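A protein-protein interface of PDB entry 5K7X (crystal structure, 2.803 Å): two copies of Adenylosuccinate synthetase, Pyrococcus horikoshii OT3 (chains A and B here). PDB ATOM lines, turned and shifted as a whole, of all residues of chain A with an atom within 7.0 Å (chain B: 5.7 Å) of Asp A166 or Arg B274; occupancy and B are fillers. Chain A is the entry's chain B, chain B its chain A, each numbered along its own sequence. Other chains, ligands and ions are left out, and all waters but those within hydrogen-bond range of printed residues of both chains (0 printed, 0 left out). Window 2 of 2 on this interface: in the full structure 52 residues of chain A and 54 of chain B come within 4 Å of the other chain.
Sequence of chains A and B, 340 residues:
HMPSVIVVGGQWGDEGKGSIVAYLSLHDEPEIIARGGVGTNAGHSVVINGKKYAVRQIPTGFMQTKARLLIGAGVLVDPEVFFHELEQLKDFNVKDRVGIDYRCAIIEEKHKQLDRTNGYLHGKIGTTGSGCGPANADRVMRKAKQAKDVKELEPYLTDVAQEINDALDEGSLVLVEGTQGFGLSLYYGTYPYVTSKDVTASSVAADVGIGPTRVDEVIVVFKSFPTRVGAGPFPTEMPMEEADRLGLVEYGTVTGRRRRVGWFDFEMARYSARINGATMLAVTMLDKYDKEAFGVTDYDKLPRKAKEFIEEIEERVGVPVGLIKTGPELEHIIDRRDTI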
ATOM      1  N   ILE A  32       6.558  22.765 -25.468  1.00  0.00           N
ATOM      2  CA  ILE A  32       6.647  21.580 -24.622  1.00  0.00           C
ATOM      3  C   ILE A  32       5.416  20.694 -24.781  1.00  0.00           C
ATOM      4  O   ILE A  32       4.338  21.170 -25.137  1.00  0.00           O
ATOM      5  CB  ILE A  32       6.809  21.956 -23.138  1.00  0.00           C
ATOM      6  CG1 ILE A  32       8.039  22.847 -22.945  1.00  0.00           C
ATOM      7  CG2 ILE A  32       6.912  20.705 -22.280  1.00  0.00           C
ATOM      8  CD1 ILE A  32       8.456  23.006 -21.500  1.00  0.00           C
ATOM      9  N   ASP A 159      14.068  18.789 -14.502  1.00  0.00           N
ATOM     10  CA  ASP A 159      12.970  19.272 -13.667  1.00  0.00           C
ATOM     11  C   ASP A 159      11.804  19.681 -14.557  1.00  0.00           C
ATOM     12  O   ASP A 159      11.762  20.806 -15.054  1.00  0.00           O
ATOM     13  CB  ASP A 159      13.422  20.456 -12.805  1.00  0.00           C
ATOM     14  CG  ASP A 159      12.426  20.807 -11.706  1.00  0.00           C
ATOM     15  OD1 ASP A 159      11.216  20.550 -11.874  1.00  0.00           O
ATOM     16  OD2 ASP A 159      12.857  21.358 -10.671  1.00  0.00           O
ATOM     17  N   VAL A 160      10.855  18.771 -14.749  1.00  0.00           N
ATOM     18  CA  VAL A 160       9.738  19.031 -15.651  1.00  0.00           C
ATOM     19  C   VAL A 160       8.874  20.172 -15.121  1.00  0.00           C
ATOM     20  O   VAL A 160       8.423  21.025 -15.887  1.00  0.00           O
ATOM     21  CB  VAL A 160       8.876  17.766 -15.863  1.00  0.00           C
ATOM     22  CG1 VAL A 160       7.620  18.096 -16.657  1.00  0.00           C
ATOM     23  CG2 VAL A 160       9.681  16.696 -16.577  1.00  0.00           C
ATOM     24  N   ALA A 161       8.691  20.208 -13.806  1.00  0.00           N
ATOM     25  CA  ALA A 161       7.910  21.257 -13.158  1.00  0.00           C
ATOM     26  C   ALA A 161       8.496  22.629 -13.465  1.00  0.00           C
ATOM     27  O   ALA A 161       7.771  23.567 -13.794  1.00  0.00           O
ATOM     28  CB  ALA A 161       7.851  21.027 -11.655  1.00  0.00           C
ATOM     29  N   GLN A 162       9.818  22.729 -13.376  1.00  0.00           N
ATOM     30  CA  GLN A 162      10.515  23.979 -13.649  1.00  0.00           C
ATOM     31  C   GLN A 162      10.425  24.368 -15.124  1.00  0.00           C
ATOM     32  O   GLN A 162      10.063  25.498 -15.448  1.00  0.00           O
ATOM     33  CB  GLN A 162      11.982  23.866 -13.232  1.00  0.00           C
ATOM     34  CG  GLN A 162      12.718  25.191 -13.152  1.00  0.00           C
ATOM     35  CD  GLN A 162      14.199  25.025 -12.868  1.00  0.00           C
ATOM     36  OE1 GLN A 162      14.776  23.967 -13.118  1.00  0.00           O
ATOM     37  NE2 GLN A 162      14.834  26.091 -12.391  1.00  0.00           N
ATOM     38  N   GLU A 163      10.754  23.429 -16.011  1.00  0.00           N
ATOM     39  CA  GLU A 163      10.725  23.675 -17.453  1.00  0.00           C
ATOM     40  C   GLU A 163       9.357  24.145 -17.935  1.00  0.00           C
ATOM     41  O   GLU A 163       9.256  25.095 -18.712  1.00  0.00           O
ATOM     42  CB  GLU A 163      11.141  22.419 -18.231  1.00  0.00           C
ATOM     43  CG  GLU A 163      12.631  22.094 -18.156  1.00  0.00           C
ATOM     44  CD  GLU A 163      13.087  21.137 -19.246  1.00  0.00           C
ATOM     45  OE1 GLU A 163      14.115  20.456 -19.046  1.00  0.00           O
ATOM     46  OE2 GLU A 163      12.423  21.067 -20.303  1.00  0.00           O
ATOM     47  N   ILE A 164       8.306  23.470 -17.479  1.00  0.00           N
ATOM     48  CA  ILE A 164       6.953  23.804 -17.908  1.00  0.00           C
ATOM     49  C   ILE A 164       6.549  25.184 -17.416  1.00  0.00           C
ATOM     50  O   ILE A 164       6.024  25.998 -18.178  1.00  0.00           O
ATOM     51  CB  ILE A 164       5.932  22.769 -17.413  1.00  0.00           C
ATOM     52  CG1 ILE A 164       6.140  21.438 -18.136  1.00  0.00           C
ATOM     53  CG2 ILE A 164       4.522  23.272 -17.638  1.00  0.00           C
ATOM     54  CD1 ILE A 164       5.078  20.413 -17.842  1.00  0.00           C
ATOM     55  N   ASN A 165       6.817  25.449 -16.143  1.00  0.00           N
ATOM     56  CA  ASN A 165       6.479  26.733 -15.557  1.00  0.00           C
ATOM     57  C   ASN A 165       7.317  27.857 -16.157  1.00  0.00           C
ATOM     58  O   ASN A 165       6.816  28.963 -16.372  1.00  0.00           O
ATOM     59  CB  ASN A 165       6.645  26.690 -14.040  1.00  0.00           C
ATOM     60  CG  ASN A 165       5.484  26.000 -13.351  1.00  0.00           C
ATOM     61  OD1 ASN A 165       4.443  26.609 -13.113  1.00  0.00           O
ATOM     62  ND2 ASN A 165       5.657  24.724 -13.027  1.00  0.00           N
ATOM     63  N   ASP A 166       8.588  27.569 -16.429  1.00  0.00           N
ATOM     64  CA  ASP A 166       9.460  28.544 -17.074  1.00  0.00           C
ATOM     65  C   ASP A 166       8.942  28.888 -18.466  1.00  0.00           C
ATOM     66  O   ASP A 166       9.027  30.033 -18.908  1.00  0.00           O
ATOM     67  CB  ASP A 166      10.892  28.014 -17.174  1.00  0.00           C
ATOM     68  CG  ASP A 166      11.657  28.137 -15.868  1.00  0.00           C
ATOM     69  OD1 ASP A 166      11.557  29.195 -15.214  1.00  0.00           O
ATOM     70  OD2 ASP A 166      12.373  27.180 -15.507  1.00  0.00           O
ATOM     71  N   ALA A 167       8.378  27.890 -19.139  1.00  0.00           N
ATOM     72  CA  ALA A 167       7.832  28.075 -20.477  1.00  0.00           C
ATOM     73  C   ALA A 167       6.557  28.908 -20.446  1.00  0.00           C
ATOM     74  O   ALA A 167       6.344  29.767 -21.303  1.00  0.00           O
ATOM     75  CB  ALA A 167       7.572  26.728 -21.135  1.00  0.00           C
ATOM     76  N   LEU A 168       5.710  28.649 -19.456  1.00  0.00           N
ATOM     77  CA  LEU A 168       4.442  29.356 -19.336  1.00  0.00           C
ATOM     78  C   LEU A 168       4.655  30.833 -19.028  1.00  0.00           C
ATOM     79  O   LEU A 168       3.782  31.662 -19.280  1.00  0.00           O
ATOM     80  CB  LEU A 168       3.581  28.712 -18.251  1.00  0.00           C
ATOM     81  CG  LEU A 168       3.029  27.343 -18.632  1.00  0.00           C
ATOM     82  CD1 LEU A 168       2.148  26.790 -17.527  1.00  0.00           C
ATOM     83  CD2 LEU A 168       2.274  27.449 -19.945  1.00  0.00           C
ATOM     84  N   ASP A 169       5.822  31.158 -18.485  1.00  0.00           N
ATOM     85  CA  ASP A 169       6.155  32.540 -18.179  1.00  0.00           C
ATOM     86  C   ASP A 169       6.537  33.300 -19.446  1.00  0.00           C
ATOM     87  O   ASP A 169       6.230  34.485 -19.582  1.00  0.00           O
ATOM     88  CB  ASP A 169       7.281  32.602 -17.144  1.00  0.00           C
ATOM     89  CG  ASP A 169       6.802  32.245 -15.749  1.00  0.00           C
ATOM     90  OD1 ASP A 169       5.569  32.210 -15.532  1.00  0.00           O
ATOM     91  OD2 ASP A 169       7.652  32.005 -14.869  1.00  0.00           O
ATOM     92  N   GLU A 170       7.191  32.611 -20.377  1.00  0.00           N
ATOM     93  CA  GLU A 170       7.612  33.236 -21.625  1.00  0.00           C
ATOM     94  C   GLU A 170       6.454  33.325 -22.614  1.00  0.00           C
ATOM     95  O   GLU A 170       6.618  33.829 -23.724  1.00  0.00           O
ATOM     96  CB  GLU A 170       8.743  32.434 -22.274  1.00  0.00           C
ATOM     97  CG  GLU A 170       9.883  32.032 -21.360  1.00  0.00           C
ATOM     98  CD  GLU A 170      10.841  31.089 -22.064  1.00  0.00           C
ATOM     99  OE1 GLU A 170      10.878  31.126 -23.312  1.00  0.00           O
ATOM    100  OE2 GLU A 170      11.533  30.303 -21.385  1.00  0.00           O
ATOM    101  N   GLY A 171       5.287  32.830 -22.210  1.00  0.00           N
ATOM    102  CA  GLY A 171       4.096  32.916 -23.035  1.00  0.00           C
ATOM    103  C   GLY A 171       3.937  31.708 -23.946  1.00  0.00           C
ATOM    104  O   GLY A 171       2.946  31.595 -24.675  1.00  0.00           O
ATOM    105  N   SER A 172       4.922  30.812 -23.915  1.00  0.00           N
ATOM    106  CA  SER A 172       4.931  29.627 -24.770  1.00  0.00           C
ATOM    107  C   SER A 172       3.741  28.710 -24.499  1.00  0.00           C
ATOM    108  O   SER A 172       3.144  28.751 -23.422  1.00  0.00           O
ATOM    109  CB  SER A 172       6.237  28.847 -24.589  1.00  0.00           C
ATOM    110  OG  SER A 172       7.367  29.664 -24.850  1.00  0.00           O
ATOM    111  N   GLY A 209       3.412  19.205 -12.736  1.00  0.00           N
ATOM    112  CA  GLY A 209       3.857  20.286 -11.874  1.00  0.00           C
ATOM    113  C   GLY A 209       3.243  21.626 -12.231  1.00  0.00           C
ATOM    114  O   GLY A 209       3.942  22.636 -12.319  1.00  0.00           O
ATOM    115  N   ILE A 210       1.928  21.636 -12.430  1.00  0.00           N
ATOM    116  CA  ILE A 210       1.208  22.846 -12.816  1.00  0.00           C
ATOM    117  C   ILE A 210       0.055  23.145 -11.863  1.00  0.00           C
ATOM    118  O   ILE A 210      -0.828  22.309 -11.668  1.00  0.00           O
ATOM    119  CB  ILE A 210       0.638  22.728 -14.239  1.00  0.00           C
ATOM    120  CG1 ILE A 210       1.760  22.591 -15.263  1.00  0.00           C
ATOM    121  CG2 ILE A 210      -0.224  23.927 -14.574  1.00  0.00           C
ATOM    122  CD1 ILE A 210       1.247  22.393 -16.670  1.00  0.00           C
ATOM    123  N   GLY A 211       0.061  24.340 -11.278  1.00  0.00           N
ATOM    124  CA  GLY A 211      -1.038  24.776 -10.434  1.00  0.00           C
ATOM    125  C   GLY A 211      -2.319  24.897 -11.235  1.00  0.00           C
ATOM    126  O   GLY A 211      -2.271  25.178 -12.430  1.00  0.00           O
ATOM    127  N   ARG A 214      -2.951  27.871 -13.474  1.00  0.00           N
ATOM    128  CA  ARG A 214      -2.102  27.985 -14.656  1.00  0.00           C
ATOM    129  C   ARG A 214      -2.653  27.195 -15.844  1.00  0.00           C
ATOM    130  O   ARG A 214      -2.100  27.255 -16.941  1.00  0.00           O
ATOM    131  CB  ARG A 214      -0.685  27.512 -14.315  1.00  0.00           C
ATOM    132  CG  ARG A 214      -0.095  28.223 -13.106  1.00  0.00           C
ATOM    133  CD  ARG A 214       0.628  29.503 -13.493  1.00  0.00           C
ATOM    134  NE  ARG A 214       1.936  29.220 -14.083  1.00  0.00           N
ATOM    135  CZ  ARG A 214       2.667  30.098 -14.766  1.00  0.00           C
ATOM    136  NH1 ARG A 214       3.853  29.742 -15.241  1.00  0.00           N
ATOM    137  NH2 ARG A 214       2.211  31.322 -14.992  1.00  0.00           N
ATOM    138  N   ALA B 269      10.545  28.477  -0.758  1.00  0.00           N
ATOM    139  CA  ALA B 269       9.276  29.188  -0.743  1.00  0.00           C
ATOM    140  C   ALA B 269       8.842  29.576  -2.153  1.00  0.00           C
ATOM    141  O   ALA B 269       7.672  29.440  -2.515  1.00  0.00           O
ATOM    142  CB  ALA B 269       9.373  30.423   0.140  1.00  0.00           C
ATOM    143  N   ARG B 270       9.796  30.053  -2.945  1.00  0.00           N
ATOM    144  CA  ARG B 270       9.516  30.487  -4.305  1.00  0.00           C
ATOM    145  C   ARG B 270       9.104  29.293  -5.156  1.00  0.00           C
ATOM    146  O   ARG B 270       8.151  29.367  -5.933  1.00  0.00           O
ATOM    147  CB  ARG B 270      10.750  31.172  -4.903  1.00  0.00           C
ATOM    148  CG  ARG B 270      10.564  31.747  -6.296  1.00  0.00           C
ATOM    149  CD  ARG B 270      11.827  32.467  -6.741  1.00  0.00           C
ATOM    150  NE  ARG B 270      11.669  33.137  -8.029  1.00  0.00           N
ATOM    151  CZ  ARG B 270      11.359  34.424  -8.161  1.00  0.00           C
ATOM    152  NH1 ARG B 270      11.189  35.177  -7.083  1.00  0.00           N
ATOM    153  NH2 ARG B 270      11.231  34.962  -9.366  1.00  0.00           N
ATOM    154  N   TYR B 271       9.814  28.185  -4.971  1.00  0.00           N
ATOM    155  CA  TYR B 271       9.538  26.954  -5.697  1.00  0.00           C
ATOM    156  C   TYR B 271       8.173  26.389  -5.328  1.00  0.00           C
ATOM    157  O   TYR B 271       7.364  26.069  -6.200  1.00  0.00           O
ATOM    158  CB  TYR B 271      10.627  25.919  -5.415  1.00  0.00           C
ATOM    159  CG  TYR B 271      10.617  24.734  -6.357  1.00  0.00           C
ATOM    160  CD1 TYR B 271       9.804  23.634  -6.116  1.00  0.00           C
ATOM    161  CD2 TYR B 271      11.426  24.715  -7.484  1.00  0.00           C
ATOM    162  CE1 TYR B 271       9.797  22.549  -6.971  1.00  0.00           C
ATOM    163  CE2 TYR B 271      11.426  23.634  -8.347  1.00  0.00           C
ATOM    164  CZ  TYR B 271      10.609  22.555  -8.085  1.00  0.00           C
ATOM    165  OH  TYR B 271      10.607  21.479  -8.941  1.00  0.00           O
ATOM    166  N   SER B 272       7.929  26.274  -4.027  1.00  0.00           N
ATOM    167  CA  SER B 272       6.669  25.756  -3.509  1.00  0.00           C
ATOM    168  C   SER B 272       5.473  26.572  -3.992  1.00  0.00           C
ATOM    169  O   SER B 272       4.438  26.021  -4.367  1.00  0.00           O
ATOM    170  CB  SER B 272       6.701  25.733  -1.984  1.00  0.00           C
ATOM    171  OG  SER B 272       5.395  25.618  -1.456  1.00  0.00           O
ATOM    172  N   ALA B 273       5.625  27.889  -3.985  1.00  0.00           N
ATOM    173  CA  ALA B 273       4.543  28.782  -4.380  1.00  0.00           C
ATOM    174  C   ALA B 273       4.239  28.655  -5.868  1.00  0.00           C
ATOM    175  O   ALA B 273       3.081  28.710  -6.282  1.00  0.00           O
ATOM    176  CB  ALA B 273       4.891  30.222  -4.035  1.00  0.00           C
ATOM    177  N   ARG B 274       5.282  28.487  -6.673  1.00  0.00           N
ATOM    178  CA  ARG B 274       5.122  28.503  -8.120  1.00  0.00           C
ATOM    179  C   ARG B 274       4.498  27.229  -8.690  1.00  0.00           C
ATOM    180  O   ARG B 274       3.629  27.296  -9.558  1.00  0.00           O
ATOM    181  CB  ARG B 274       6.484  28.727  -8.779  1.00  0.00           C
ATOM    182  CG  ARG B 274       6.409  28.974 -10.266  1.00  0.00           C
ATOM    183  CD  ARG B 274       7.791  28.964 -10.885  1.00  0.00           C
ATOM    184  NE  ARG B 274       7.771  29.495 -12.242  1.00  0.00           N
ATOM    185  CZ  ARG B 274       8.806  29.453 -13.072  1.00  0.00           C
ATOM    186  NH1 ARG B 274       8.702  29.969 -14.287  1.00  0.00           N
ATOM    187  NH2 ARG B 274       9.939  28.880 -12.693  1.00  0.00           N
ATOM    188  N   ILE B 275       4.941  26.074  -8.203  1.00  0.00           N
ATOM    189  CA  ILE B 275       4.374  24.796  -8.625  1.00  0.00           C
ATOM    190  C   ILE B 275       2.904  24.674  -8.199  1.00  0.00           C
ATOM    191  O   ILE B 275       2.084  24.091  -8.913  1.00  0.00           O
ATOM    192  CB  ILE B 275       5.211  23.608  -8.075  1.00  0.00           C
ATOM    193  CG1 ILE B 275       6.405  23.325  -8.994  1.00  0.00           C
ATOM    194  CG2 ILE B 275       4.377  22.346  -7.973  1.00  0.00           C
ATOM    195  CD1 ILE B 275       7.498  24.377  -8.966  1.00  0.00           C
ATOM    196  N   ASN B 276       2.571  25.255  -7.049  1.00  0.00           N
ATOM    197  CA  ASN B 276       1.186  25.301  -6.591  1.00  0.00           C
ATOM    198  C   ASN B 276       0.323  26.238  -7.427  1.00  0.00           C
ATOM    199  O   ASN B 276      -0.905  26.174  -7.374  1.00  0.00           O
ATOM    200  CB  ASN B 276       1.111  25.729  -5.123  1.00  0.00           C
ATOM    201  CG  ASN B 276       1.037  24.551  -4.179  1.00  0.00           C
ATOM    202  OD1 ASN B 276       0.026  23.852  -4.129  1.00  0.00           O
ATOM    203  ND2 ASN B 276       2.100  24.331  -3.411  1.00  0.00           N
ATOM    204  N   GLY B 277       0.968  27.111  -8.194  1.00  0.00           N
ATOM    205  CA  GLY B 277       0.245  28.104  -8.964  1.00  0.00           C
ATOM    206  C   GLY B 277      -0.395  29.120  -8.040  1.00  0.00           C
ATOM    207  O   GLY B 277      -1.544  29.519  -8.229  1.00  0.00           O
ATOM    208  N   ALA B 278       0.363  29.540  -7.032  1.00  0.00           N
ATOM    209  CA  ALA B 278      -0.139  30.447  -6.009  1.00  0.00           C
ATOM    210  C   ALA B 278      -0.549  31.798  -6.580  1.00  0.00           C
ATOM    211  O   ALA B 278       0.193  32.412  -7.349  1.00  0.00           O
ATOM    212  CB  ALA B 278       0.904  30.636  -4.925  1.00  0.00           C
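O of Ser B272 is in hydrogen-bond range of ND2 of Asn B276 (3.0 Å).
OD1 of Asp A159 is in hydrogen-bond range of N of Ala A161, at 3.2 Å.
The side-chain carboxylate (OD1) of Asp A159 is in hydrogen-bond range of the backbone NH (N) of Gln A162 (3.0 Å).
O of Ala A161 is in hydrogen-bond range of ND2 of Asn A165 (2.5 Å).
The backbone carbonyl oxygen (O) of Asn A165 lies within hydrogen-bond range of the guanidinium group (NH1) of Arg A214, 3.3 Å away.
The side-chain carboxylate (OD1) of Asp A169 is in salt-bridge range of the guanidinium group (NH1) of Arg A214, 3.0 Å away.
Of the 10 printed residues of chain B, 5 touch a printed residue of chain A.
Printed residues of chain B that touch a printed residue of chain A: Tyr B271, Arg B274, Ile B275, Asn B276 and Gly B277.
Hydrophobic or aromatic side chains of chain B that line the printed part of chain A: Tyr B271 and Ile B275.
Hydrophobic or aromatic side chains of chain A that line the printed part of chain B: Ala A161.
Along chain A the printed residues that touch a printed residue of chain B span positions 159 to 211.
Among the printed residues, Asp or Glu carboxylates within 4 Å of a Lys or Arg side-chain nitrogen of the other chain: Asp A166 with Arg B274 (3.0 Å) and Asp A169 with Arg B274 (2.4 Å).
Among the printed residues, pairs that only touch across the chains: Ala A161 with Tyr B271 (3.9 Å), Ala A161 with Ile B275 (3.8 Å), Ile A210 with Ile B275 (3.7 Å), Gly A211 with Asn B276 (3.4 Å) and Gly A211 with Gly B277 (3.8 Å).
OD2 of Asp A159 is in hydrogen-bond range of OH of Tyr B271.
The guanidinium group (NH1) of Arg B274 lies within hydrogen-bond range of the backbone carbonyl oxygen (O) of Asn A165 (3.0 Å).
The guanidinium group (NH2) of Arg B274 is in salt-bridge range of the side-chain carboxylate (OD1) of Asp A166, 3.0 Å away.
The guanidinium group (NE) of Arg B274 lies within salt-bridge range of the side-chain carboxylate (OD2) of Asp A169.
O of Ile B275 sits at hydrogen-bond distance from N of Gly A211, 3.1 Å away.
No position is printed for both chains.
Of the 10 pairs that touch across the chains among the printed residues, none has its exchanged pair printed and touching as well.
Asp A166 touches just one residue of chain B: Arg B274.
Of the printed residues of chain A, Arg B274 touches Asn A165 (3.0 Å), Asp A166 (3.0 Å) and Asp A169 (2.4 Å).
Of the printed residues of chain B, Gly A211 touches Ile B275 (3.1 Å), Asn B276 (3.4 Å) and Gly B277 (3.8 Å).
Of the printed residues of chain B, Asp A169 touches Arg B274 (2.4 Å).
Of the printed residues of chain B, Asn A165 touches Arg B274.
Of the printed residues of chain B, Ile A210 touches Ile B275.
Ile A32 touches none of the printed residues of chain B.
Ser A172 touches none of the printed residues of chain B.
The nearest printed residue of chain B that does not touch Asp A166 is Tyr B271 (8.0 Å).
The nearest printed residue of chain A that does not touch Ile B275 is Gly A209 (4.1 Å).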
